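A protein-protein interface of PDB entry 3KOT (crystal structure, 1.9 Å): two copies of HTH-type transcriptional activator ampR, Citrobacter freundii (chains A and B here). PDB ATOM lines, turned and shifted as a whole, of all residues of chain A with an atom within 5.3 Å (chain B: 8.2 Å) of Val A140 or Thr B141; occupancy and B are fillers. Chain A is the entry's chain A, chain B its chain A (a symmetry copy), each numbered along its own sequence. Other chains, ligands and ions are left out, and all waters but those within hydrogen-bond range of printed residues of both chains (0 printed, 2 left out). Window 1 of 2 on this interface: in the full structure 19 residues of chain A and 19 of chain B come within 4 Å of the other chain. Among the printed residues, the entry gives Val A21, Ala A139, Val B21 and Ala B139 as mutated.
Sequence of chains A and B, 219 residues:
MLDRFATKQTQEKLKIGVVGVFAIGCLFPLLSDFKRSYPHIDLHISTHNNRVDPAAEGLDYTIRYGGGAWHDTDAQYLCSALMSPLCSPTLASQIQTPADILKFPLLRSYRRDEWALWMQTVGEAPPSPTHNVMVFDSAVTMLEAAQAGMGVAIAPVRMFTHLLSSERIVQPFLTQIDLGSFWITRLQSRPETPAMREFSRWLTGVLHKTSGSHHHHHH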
ATOM      1  N   GLY A  20     -14.625  14.734  -2.017  1.00  0.00           N
ATOM      2  CA  GLY A  20     -15.570  15.733  -2.472  1.00  0.00           C
ATOM      3  C   GLY A  20     -14.934  17.028  -2.945  1.00  0.00           C
ATOM      4  O   GLY A  20     -15.277  17.541  -4.002  1.00  0.00           O
ATOM      5  N   VAL A  21     -14.015  17.579  -2.160  1.00  0.00           N
ATOM      6  CA  VAL A  21     -13.397  18.853  -2.552  1.00  0.00           C
ATOM      7  C   VAL A  21     -12.719  18.754  -3.937  1.00  0.00           C
ATOM      8  O   VAL A  21     -12.741  19.704  -4.712  1.00  0.00           O
ATOM      9  CB  VAL A  21     -12.409  19.385  -1.466  1.00  0.00           C
ATOM     10  CG1 VAL A  21     -11.249  18.411  -1.247  1.00  0.00           C
ATOM     11  CG2 VAL A  21     -11.903  20.770  -1.821  1.00  0.00           C
ATOM     12  N   ILE A  24     -15.640  18.408  -6.864  1.00  0.00           N
ATOM     13  CA  ILE A  24     -16.232  19.702  -7.241  1.00  0.00           C
ATOM     14  C   ILE A  24     -15.220  20.712  -7.814  1.00  0.00           C
ATOM     15  O   ILE A  24     -15.532  21.470  -8.745  1.00  0.00           O
ATOM     16  CB  ILE A  24     -16.952  20.350  -6.045  1.00  0.00           C
ATOM     17  CG1 ILE A  24     -17.991  19.381  -5.469  1.00  0.00           C
ATOM     18  CG2 ILE A  24     -17.577  21.688  -6.460  1.00  0.00           C
ATOM     19  CD1 ILE A  24     -19.082  18.941  -6.451  1.00  0.00           C
ATOM     20  N   THR A  47     -18.448   9.989  -4.160  1.00  0.00           N
ATOM     21  CA  THR A  47     -17.638  10.926  -3.387  1.00  0.00           C
ATOM     22  C   THR A  47     -17.473  10.438  -1.943  1.00  0.00           C
ATOM     23  O   THR A  47     -18.273   9.643  -1.441  1.00  0.00           O
ATOM     24  CB  THR A  47     -18.182  12.388  -3.416  1.00  0.00           C
ATOM     25  OG1 THR A  47     -19.401  12.486  -2.667  1.00  0.00           O
ATOM     26  CG2 THR A  47     -18.417  12.890  -4.851  1.00  0.00           C
ATOM     27  N   SER A 138     -15.442  17.805   5.783  1.00  0.00           N
ATOM     28  CA  SER A 138     -15.338  18.072   4.355  1.00  0.00           C
ATOM     29  C   SER A 138     -15.067  19.543   4.097  1.00  0.00           C
ATOM     30  O   SER A 138     -15.784  20.404   4.617  1.00  0.00           O
ATOM     31  CB  SER A 138     -16.651  17.686   3.674  1.00  0.00           C
ATOM     32  OG  SER A 138     -16.709  18.218   2.352  1.00  0.00           O
ATOM     33  N   ALA A 139     -14.048  19.831   3.289  1.00  0.00           N
ATOM     34  CA  ALA A 139     -13.765  21.204   2.867  1.00  0.00           C
ATOM     35  C   ALA A 139     -14.914  21.834   2.091  1.00  0.00           C
ATOM     36  O   ALA A 139     -15.059  23.063   2.068  1.00  0.00           O
ATOM     37  CB  ALA A 139     -12.475  21.269   2.036  1.00  0.00           C
ATOM     38  N   VAL A 140     -15.725  21.009   1.436  1.00  0.00           N
ATOM     39  CA  VAL A 140     -16.862  21.551   0.697  1.00  0.00           C
ATOM     40  C   VAL A 140     -17.833  22.164   1.707  1.00  0.00           C
ATOM     41  O   VAL A 140     -18.298  23.298   1.540  1.00  0.00           O
ATOM     42  CB  VAL A 140     -17.540  20.472  -0.174  1.00  0.00           C
ATOM     43  CG1 VAL A 140     -18.748  21.048  -0.965  1.00  0.00           C
ATOM     44  CG2 VAL A 140     -16.512  19.872  -1.138  1.00  0.00           C
ATOM     45  N   THR A 141     -18.099  21.432   2.784  1.00  0.00           N
ATOM     46  CA  THR A 141     -18.993  21.924   3.837  1.00  0.00           C
ATOM     47  C   THR A 141     -18.393  23.140   4.561  1.00  0.00           C
ATOM     48  O   THR A 141     -19.073  24.133   4.797  1.00  0.00           O
ATOM     49  CB  THR A 141     -19.345  20.785   4.818  1.00  0.00           C
ATOM     50  OG1 THR A 141     -19.946  19.718   4.072  1.00  0.00           O
ATOM     51  CG2 THR A 141     -20.317  21.257   5.932  1.00  0.00           C
ATOM     52  N   MET A 142     -17.110  23.056   4.894  1.00  0.00           N
ATOM     53  CA  MET A 142     -16.396  24.200   5.458  1.00  0.00           C
ATOM     54  C   MET A 142     -16.611  25.476   4.639  1.00  0.00           C
ATOM     55  O   MET A 142     -16.906  26.526   5.201  1.00  0.00           O
ATOM     56  CB  MET A 142     -14.899  23.927   5.515  1.00  0.00           C
ATOM     57  CG  MET A 142     -14.117  25.032   6.160  1.00  0.00           C
ATOM     58  SD  MET A 142     -12.351  24.842   5.895  1.00  0.00           S
ATOM     59  CE  MET A 142     -12.001  23.415   6.920  1.00  0.00           C
ATOM     60  N   LEU A 143     -16.430  25.393   3.324  1.00  0.00           N
ATOM     61  CA  LEU A 143     -16.517  26.592   2.486  1.00  0.00           C
ATOM     62  C   LEU A 143     -17.964  27.080   2.330  1.00  0.00           C
ATOM     63  O   LEU A 143     -18.194  28.242   2.053  1.00  0.00           O
ATOM     64  CB  LEU A 143     -15.846  26.400   1.117  1.00  0.00           C
ATOM     65  CG  LEU A 143     -14.368  26.828   1.072  1.00  0.00           C
ATOM     66  CD1 LEU A 143     -14.227  28.342   1.272  1.00  0.00           C
ATOM     67  CD2 LEU A 143     -13.555  26.067   2.130  1.00  0.00           C
ATOM     68  N   GLU A 144     -18.932  26.191   2.492  1.00  0.00           N
ATOM     69  CA  GLU A 144     -20.311  26.643   2.551  1.00  0.00           C
ATOM     70  C   GLU A 144     -20.523  27.495   3.813  1.00  0.00           C
ATOM     71  O   GLU A 144     -21.112  28.580   3.749  1.00  0.00           O
ATOM     72  CB  GLU A 144     -21.271  25.457   2.487  1.00  0.00           C
ATOM     73  CG  GLU A 144     -21.366  24.864   1.090  1.00  0.00           C
ATOM     74  CD  GLU A 144     -21.845  25.897   0.069  1.00  0.00           C
ATOM     75  OE1 GLU A 144     -22.969  26.425   0.256  1.00  0.00           O
ATOM     76  OE2 GLU A 144     -21.094  26.192  -0.898  1.00  0.00           O
ATOM     77  N   PHE A 160     -11.203  25.833  -4.981  1.00  0.00           N
ATOM     78  CA  PHE A 160     -12.318  26.768  -4.826  1.00  0.00           C
ATOM     79  C   PHE A 160     -12.252  27.969  -5.769  1.00  0.00           C
ATOM     80  O   PHE A 160     -12.787  29.036  -5.481  1.00  0.00           O
ATOM     81  CB  PHE A 160     -12.475  27.191  -3.358  1.00  0.00           C
ATOM     82  CG  PHE A 160     -12.814  26.046  -2.459  1.00  0.00           C
ATOM     83  CD1 PHE A 160     -14.109  25.546  -2.413  1.00  0.00           C
ATOM     84  CD2 PHE A 160     -11.831  25.427  -1.698  1.00  0.00           C
ATOM     85  CE1 PHE A 160     -14.420  24.451  -1.610  1.00  0.00           C
ATOM     86  CE2 PHE A 160     -12.138  24.343  -0.888  1.00  0.00           C
ATOM     87  CZ  PHE A 160     -13.440  23.860  -0.844  1.00  0.00           C
ATOM     88  N   GLY B  20     -23.580  17.304   7.819  1.00  0.00           N
ATOM     89  CA  GLY B  20     -23.286  18.527   7.100  1.00  0.00           C
ATOM     90  C   GLY B  20     -24.506  19.222   6.521  1.00  0.00           C
ATOM     91  O   GLY B  20     -24.666  20.426   6.671  1.00  0.00           O
ATOM     92  N   VAL B  21     -25.367  18.476   5.839  1.00  0.00           N
ATOM     93  CA  VAL B  21     -26.544  19.106   5.225  1.00  0.00           C
ATOM     94  C   VAL B  21     -27.408  19.841   6.274  1.00  0.00           C
ATOM     95  O   VAL B  21     -27.972  20.893   5.992  1.00  0.00           O
ATOM     96  CB  VAL B  21     -27.389  18.090   4.396  1.00  0.00           C
ATOM     97  CG1 VAL B  21     -27.935  16.968   5.283  1.00  0.00           C
ATOM     98  CG2 VAL B  21     -28.507  18.791   3.648  1.00  0.00           C
ATOM     99  N   ILE B  24     -25.371  23.200   7.610  1.00  0.00           N
ATOM    100  CA  ILE B  24     -25.494  24.348   6.697  1.00  0.00           C
ATOM    101  C   ILE B  24     -26.942  24.828   6.484  1.00  0.00           C
ATOM    102  O   ILE B  24     -27.206  26.035   6.377  1.00  0.00           O
ATOM    103  CB  ILE B  24     -24.872  24.034   5.325  1.00  0.00           C
ATOM    104  CG1 ILE B  24     -23.417  23.583   5.499  1.00  0.00           C
ATOM    105  CG2 ILE B  24     -24.994  25.246   4.393  1.00  0.00           C
ATOM    106  CD1 ILE B  24     -22.497  24.607   6.173  1.00  0.00           C
ATOM    107  N   THR B  47     -18.686  18.397  11.890  1.00  0.00           N
ATOM    108  CA  THR B  47     -19.621  17.886  10.891  1.00  0.00           C
ATOM    109  C   THR B  47     -19.228  16.471  10.453  1.00  0.00           C
ATOM    110  O   THR B  47     -18.074  16.056  10.590  1.00  0.00           O
ATOM    111  CB  THR B  47     -19.781  18.823   9.654  1.00  0.00           C
ATOM    112  OG1 THR B  47     -18.587  18.812   8.858  1.00  0.00           O
ATOM    113  CG2 THR B  47     -20.116  20.267  10.061  1.00  0.00           C
ATOM    114  N   ASN B  49     -20.692  13.034   7.514  1.00  0.00           N
ATOM    115  CA  ASN B  49     -21.463  12.783   6.301  1.00  0.00           C
ATOM    116  C   ASN B  49     -22.600  11.781   6.504  1.00  0.00           C
ATOM    117  O   ASN B  49     -23.046  11.126   5.556  1.00  0.00           O
ATOM    118  CB  ASN B  49     -20.558  12.406   5.122  1.00  0.00           C
ATOM    119  CG  ASN B  49     -19.826  11.083   5.320  1.00  0.00           C
ATOM    120  OD1 ASN B  49     -20.055  10.364   6.295  1.00  0.00           O
ATOM    121  ND2 ASN B  49     -18.941  10.755   4.383  1.00  0.00           N
ATOM    122  N   LEU B 107     -28.185  12.377  -9.677  1.00  0.00           N
ATOM    123  CA  LEU B 107     -27.289  12.444  -8.535  1.00  0.00           C
ATOM    124  C   LEU B 107     -28.031  11.850  -7.336  1.00  0.00           C
ATOM    125  O   LEU B 107     -29.182  12.214  -7.081  1.00  0.00           O
ATOM    126  CB  LEU B 107     -26.884  13.898  -8.258  1.00  0.00           C
ATOM    127  CG  LEU B 107     -26.544  14.744  -9.497  1.00  0.00           C
ATOM    128  CD1 LEU B 107     -26.283  16.213  -9.149  1.00  0.00           C
ATOM    129  CD2 LEU B 107     -25.350  14.137 -10.287  1.00  0.00           C
ATOM    130  N   VAL B 135     -22.777   9.291  -7.309  1.00  0.00           N
ATOM    131  CA  VAL B 135     -23.113   8.964  -5.927  1.00  0.00           C
ATOM    132  C   VAL B 135     -22.348   9.854  -4.951  1.00  0.00           C
ATOM    133  O   VAL B 135     -21.134  10.038  -5.088  1.00  0.00           O
ATOM    134  CB  VAL B 135     -22.781   7.475  -5.648  1.00  0.00           C
ATOM    135  CG1 VAL B 135     -23.137   7.080  -4.211  1.00  0.00           C
ATOM    136  CG2 VAL B 135     -23.483   6.580  -6.678  1.00  0.00           C
ATOM    137  N   PHE B 136     -23.065  10.397  -3.965  1.00  0.00           N
ATOM    138  CA  PHE B 136     -22.524  11.386  -3.039  1.00  0.00           C
ATOM    139  C   PHE B 136     -22.634  10.982  -1.582  1.00  0.00           C
ATOM    140  O   PHE B 136     -23.713  10.592  -1.121  1.00  0.00           O
ATOM    141  CB  PHE B 136     -23.263  12.710  -3.257  1.00  0.00           C
ATOM    142  CG  PHE B 136     -23.002  13.306  -4.605  1.00  0.00           C
ATOM    143  CD1 PHE B 136     -21.968  14.207  -4.781  1.00  0.00           C
ATOM    144  CD2 PHE B 136     -23.741  12.908  -5.704  1.00  0.00           C
ATOM    145  CE1 PHE B 136     -21.701  14.727  -6.015  1.00  0.00           C
ATOM    146  CE2 PHE B 136     -23.484  13.433  -6.953  1.00  0.00           C
ATOM    147  CZ  PHE B 136     -22.475  14.350  -7.115  1.00  0.00           C
ATOM    148  N   ASP B 137     -21.518  11.095  -0.858  1.00  0.00           N
ATOM    149  CA  ASP B 137     -21.499  10.811   0.569  1.00  0.00           C
ATOM    150  C   ASP B 137     -22.258  11.900   1.301  1.00  0.00           C
ATOM    151  O   ASP B 137     -22.712  11.707   2.418  1.00  0.00           O
ATOM    152  CB  ASP B 137     -20.058  10.741   1.100  1.00  0.00           C
ATOM    153  CG  ASP B 137     -19.365  12.084   1.080  1.00  0.00           C
ATOM    154  OD1 ASP B 137     -19.340  12.729   0.006  1.00  0.00           O
ATOM    155  OD2 ASP B 137     -18.832  12.501   2.131  1.00  0.00           O
ATOM    156  N   SER B 138     -22.415  13.046   0.644  1.00  0.00           N
ATOM    157  CA  SER B 138     -22.944  14.232   1.305  1.00  0.00           C
ATOM    158  C   SER B 138     -23.872  14.999   0.381  1.00  0.00           C
ATOM    159  O   SER B 138     -23.497  15.305  -0.756  1.00  0.00           O
ATOM    160  CB  SER B 138     -21.786  15.144   1.709  1.00  0.00           C
ATOM    161  OG  SER B 138     -22.263  16.439   2.066  1.00  0.00           O
ATOM    162  N   ALA B 139     -25.070  15.321   0.868  1.00  0.00           N
ATOM    163  CA  ALA B 139     -26.003  16.164   0.118  1.00  0.00           C
ATOM    164  C   ALA B 139     -25.445  17.552  -0.172  1.00  0.00           C
ATOM    165  O   ALA B 139     -25.851  18.205  -1.142  1.00  0.00           O
ATOM    166  CB  ALA B 139     -27.346  16.284   0.852  1.00  0.00           C
ATOM    167  N   VAL B 140     -24.530  18.024   0.671  1.00  0.00           N
ATOM    168  CA  VAL B 140     -23.937  19.336   0.430  1.00  0.00           C
ATOM    169  C   VAL B 140     -23.122  19.257  -0.862  1.00  0.00           C
ATOM    170  O   VAL B 140     -23.241  20.114  -1.746  1.00  0.00           O
ATOM    171  CB  VAL B 140     -23.079  19.800   1.626  1.00  0.00           C
ATOM    172  CG1 VAL B 140     -22.450  21.199   1.374  1.00  0.00           C
ATOM    173  CG2 VAL B 140     -23.938  19.824   2.893  1.00  0.00           C
ATOM    174  N   THR B 141     -22.330  18.197  -0.992  1.00  0.00           N
ATOM    175  CA  THR B 141     -21.522  17.995  -2.199  1.00  0.00           C
ATOM    176  C   THR B 141     -22.405  17.743  -3.431  1.00  0.00           C
ATOM    177  O   THR B 141     -22.183  18.314  -4.494  1.00  0.00           O
ATOM    178  CB  THR B 141     -20.503  16.857  -1.977  1.00  0.00           C
ATOM    179  OG1 THR B 141     -19.688  17.196  -0.846  1.00  0.00           O
ATOM    180  CG2 THR B 141     -19.603  16.632  -3.221  1.00  0.00           C
ATOM    181  N   MET B 142     -23.414  16.894  -3.272  1.00  0.00           N
ATOM    182  CA  MET B 142     -24.402  16.684  -4.329  1.00  0.00           C
ATOM    183  C   MET B 142     -24.947  18.004  -4.882  1.00  0.00           C
ATOM    184  O   MET B 142     -25.014  18.185  -6.093  1.00  0.00           O
ATOM    185  CB  MET B 142     -25.580  15.869  -3.812  1.00  0.00           C
ATOM    186  CG  MET B 142     -26.592  15.549  -4.872  1.00  0.00           C
ATOM    187  SD  MET B 142     -28.114  14.907  -4.167  1.00  0.00           S
ATOM    188  CE  MET B 142     -27.574  13.300  -3.589  1.00  0.00           C
ATOM    189  N   LEU B 143     -25.369  18.905  -3.999  1.00  0.00           N
ATOM    190  CA  LEU B 143     -25.998  20.149  -4.451  1.00  0.00           C
ATOM    191  C   LEU B 143     -24.978  21.118  -5.065  1.00  0.00           C
ATOM    192  O   LEU B 143     -25.339  21.973  -5.852  1.00  0.00           O
ATOM    193  CB  LEU B 143     -26.813  20.831  -3.340  1.00  0.00           C
ATOM    194  CG  LEU B 143     -28.298  20.430  -3.310  1.00  0.00           C
ATOM    195  CD1 LEU B 143     -29.027  20.919  -4.568  1.00  0.00           C
ATOM    196  CD2 LEU B 143     -28.442  18.908  -3.162  1.00  0.00           C
ATOM    197  N   GLU B 144     -23.713  20.995  -4.692  1.00  0.00           N
ATOM    198  CA  GLU B 144     -22.689  21.752  -5.389  1.00  0.00           C
ATOM    199  C   GLU B 144     -22.583  21.263  -6.843  1.00  0.00           C
ATOM    200  O   GLU B 144     -22.549  22.070  -7.778  1.00  0.00           O
ATOM    201  CB  GLU B 144     -21.355  21.662  -4.652  1.00  0.00           C
ATOM    202  CG  GLU B 144     -21.334  22.508  -3.388  1.00  0.00           C
ATOM    203  CD  GLU B 144     -21.590  23.984  -3.693  1.00  0.00           C
ATOM    204  OE1 GLU B 144     -20.792  24.568  -4.467  1.00  0.00           O
ATOM    205  OE2 GLU B 144     -22.593  24.548  -3.179  1.00  0.00           O
ATOM    206  N   ALA B 145     -22.561  19.943  -7.021  1.00  0.00           N
ATOM    207  CA  ALA B 145     -22.568  19.335  -8.347  1.00  0.00           C
ATOM    208  C   ALA B 145     -23.817  19.726  -9.143  1.00  0.00           C
ATOM    209  O   ALA B 145     -23.735  19.999 -10.340  1.00  0.00           O
ATOM    210  CB  ALA B 145     -22.466  17.815  -8.237  1.00  0.00           C
ATOM    211  N   ALA B 146     -24.968  19.735  -8.474  1.00  0.00           N
ATOM    212  CA  ALA B 146     -26.223  20.102  -9.123  1.00  0.00           C
ATOM    213  C   ALA B 146     -26.202  21.549  -9.624  1.00  0.00           C
ATOM    214  O   ALA B 146     -26.638  21.824 -10.743  1.00  0.00           O
ATOM    215  CB  ALA B 146     -27.409  19.878  -8.173  1.00  0.00           C
ATOM    216  N   GLN B 147     -25.717  22.470  -8.788  1.00  0.00           N
ATOM    217  CA  GLN B 147     -25.607  23.883  -9.181  1.00  0.00           C
ATOM    218  C   GLN B 147     -24.784  24.046 -10.443  1.00  0.00           C
ATOM    219  O   GLN B 147     -25.075  24.906 -11.280  1.00  0.00           O
ATOM    220  CB  GLN B 147     -24.972  24.725  -8.070  1.00  0.00           C
ATOM    221  CG  GLN B 147     -25.891  24.995  -6.899  1.00  0.00           C
ATOM    222  CD  GLN B 147     -25.159  25.648  -5.763  1.00  0.00           C
ATOM    223  OE1 GLN B 147     -24.883  26.840  -5.788  1.00  0.00           O
ATOM    224  NE2 GLN B 147     -24.810  24.858  -4.768  1.00  0.00           N
ATOM    225  N   ALA B 148     -23.741  23.241 -10.566  1.00  0.00           N
ATOM    226  CA  ALA B 148     -22.866  23.297 -11.734  1.00  0.00           C
ATOM    227  C   ALA B 148     -23.457  22.550 -12.929  1.00  0.00           C
ATOM    228  O   ALA B 148     -22.785  22.368 -13.940  1.00  0.00           O
ATOM    229  CB  ALA B 148     -21.492  22.737 -11.385  1.00  0.00           C
ATOM    230  N   MET B 150     -24.309  19.304 -13.203  1.00  0.00           N
ATOM    231  CA  MET B 150     -23.747  17.969 -13.417  1.00  0.00           C
ATOM    232  C   MET B 150     -24.865  16.921 -13.530  1.00  0.00           C
ATOM    233  O   MET B 150     -24.675  15.837 -14.074  1.00  0.00           O
ATOM    234  CB  MET B 150     -22.766  17.598 -12.291  1.00  0.00           C
ATOM    235  CG  MET B 150     -21.440  18.402 -12.266  1.00  0.00           C
ATOM    236  SD  MET B 150     -20.507  18.221 -13.802  1.00  0.00           S
ATOM    237  CE  MET B 150     -20.256  16.449 -13.842  1.00  0.00           C
ATOM    238  N   ALA B 153     -30.316  16.459  -8.786  1.00  0.00           N
ATOM    239  CA  ALA B 153     -30.133  15.930  -7.441  1.00  0.00           C
ATOM    240  C   ALA B 153     -31.479  15.535  -6.846  1.00  0.00           C
ATOM    241  O   ALA B 153     -32.515  15.991  -7.310  1.00  0.00           O
ATOM    242  CB  ALA B 153     -29.465  16.990  -6.555  1.00  0.00           C
ATOM    243  N   PHE B 160     -32.011  23.293   1.757  1.00  0.00           N
ATOM    244  CA  PHE B 160     -31.403  24.086   0.688  1.00  0.00           C
ATOM    245  C   PHE B 160     -32.190  25.347   0.332  1.00  0.00           C
ATOM    246  O   PHE B 160     -32.116  25.850  -0.786  1.00  0.00           O
ATOM    247  CB  PHE B 160     -31.114  23.215  -0.542  1.00  0.00           C
ATOM    248  CG  PHE B 160     -30.122  22.131  -0.265  1.00  0.00           C
ATOM    249  CD1 PHE B 160     -28.765  22.419  -0.198  1.00  0.00           C
ATOM    250  CD2 PHE B 160     -30.543  20.833  -0.012  1.00  0.00           C
ATOM    251  CE1 PHE B 160     -27.841  21.422   0.104  1.00  0.00           C
ATOM    252  CE2 PHE B 160     -29.625  19.833   0.278  1.00  0.00           C
ATOM    253  CZ  PHE B 160     -28.269  20.134   0.331  1.00  0.00           C
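Thr B141 touches Ile A24 (O to CD1, 3.7 Å). CD1 of Ile A24 touches CB of Glu B144, 3.98 Å away. Ala B145 touches Ile A24 (N to CD1, 3.7 Å). Thr A47 touches Phe B136. Val A140 touches Thr B141. CG1 of Val A140 touches CG of Glu B144, 3.8 Å away. O of Thr A141 touches CD1 of Ile B24, 3.7 Å away. Thr A141 touches Val B140. CB of Glu A144 touches CD1 of Ile B24, at 3.98 Å. Val B140 touches Glu A144 (CG1 to CG, 3.8 Å).
The side-chain hydroxyl of Thr A47 is in hydrogen-bond range of the side-chain carboxylate of Asp B137, at 2.7 Å. OE2 of Glu B144 sits close to OE2 of Glu A144 (3.2 Å). The backbone carbonyl oxygen of Val B135 sits at hydrogen-bond distance from the backbone NH of Thr A47 (2.8 Å).
Ile A24 touches Thr B141, and with the chains exchanged Thr A141 touches Ile B24. Ile A24 touches Glu B144, and with the chains exchanged Glu A144 touches Ile B24. Val A140 touches Thr B141, and with the chains exchanged Thr A141 touches Val B140. Glu B144 touches its own counterpart, Glu A144. 12 positions are printed for both chains. Of the 13 pairs that touch across the chains among the printed residues, 9 have their exchanged pair printed and touching as well.
No residue of chain B comes within 4 Å of Ala A139. Of the printed residues of chain B, Ile A24 touches Thr B141 (3.7 Å), Glu B144 (3.98 Å) and Ala B145 (3.7 Å). Printed residues of chain B within 4 Å of Glu A144: Ile B24, Val B140 and Glu B144. Of the printed residues of chain A, Ala B145 touches Ile A24. Of the printed residues of chain A, Phe B136 touches Thr A47 (3.3 Å). Printed residues of chain B within 4 Å of Thr A47: Val B135 (2.8 Å), Phe B136 (3.3 Å) and Asp B137 (2.7 Å). Met B150 touches none of the printed residues of chain A. Met B142 touches none of the printed residues of chain A. The nearest printed residue of chain A that does not touch Thr B141 is Thr A47 (4.2 Å).
The side-chain carboxylate (OE2) of Glu B144 lies within hydrogen-bond range of the side-chain amide nitrogen (NE2) of Gln B147. The side-chain hydroxyl (OG) of Ser B138 is in hydrogen-bond range of the backbone NH (N) of Val B140 (3.1 Å). The backbone carbonyl oxygen (O) of Ala B145 lies within hydrogen-bond range of the backbone NH (N) of Met B150. OD2 of Asp B137 is in hydrogen-bond range of ND2 of Asn B49, at 2.9 Å. OG of Ser A138 lies within hydrogen-bond range of N of Val A140 (3.1 Å).
Hydrophobic or aromatic side chains of chain A within 4 Å of the printed part of chain B: Ile A24 and Val A140. Hydrophobic or aromatic side chains of chain B that line the printed part of chain A: Ile B24, Phe B136, Val B140 and Ala B145. Among the printed residues, 13 pairs touch across the chains. Among the printed residues, no Asp or Glu carboxylate lies within 4 Å of a Lys or Arg side-chain nitrogen of the other chain.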
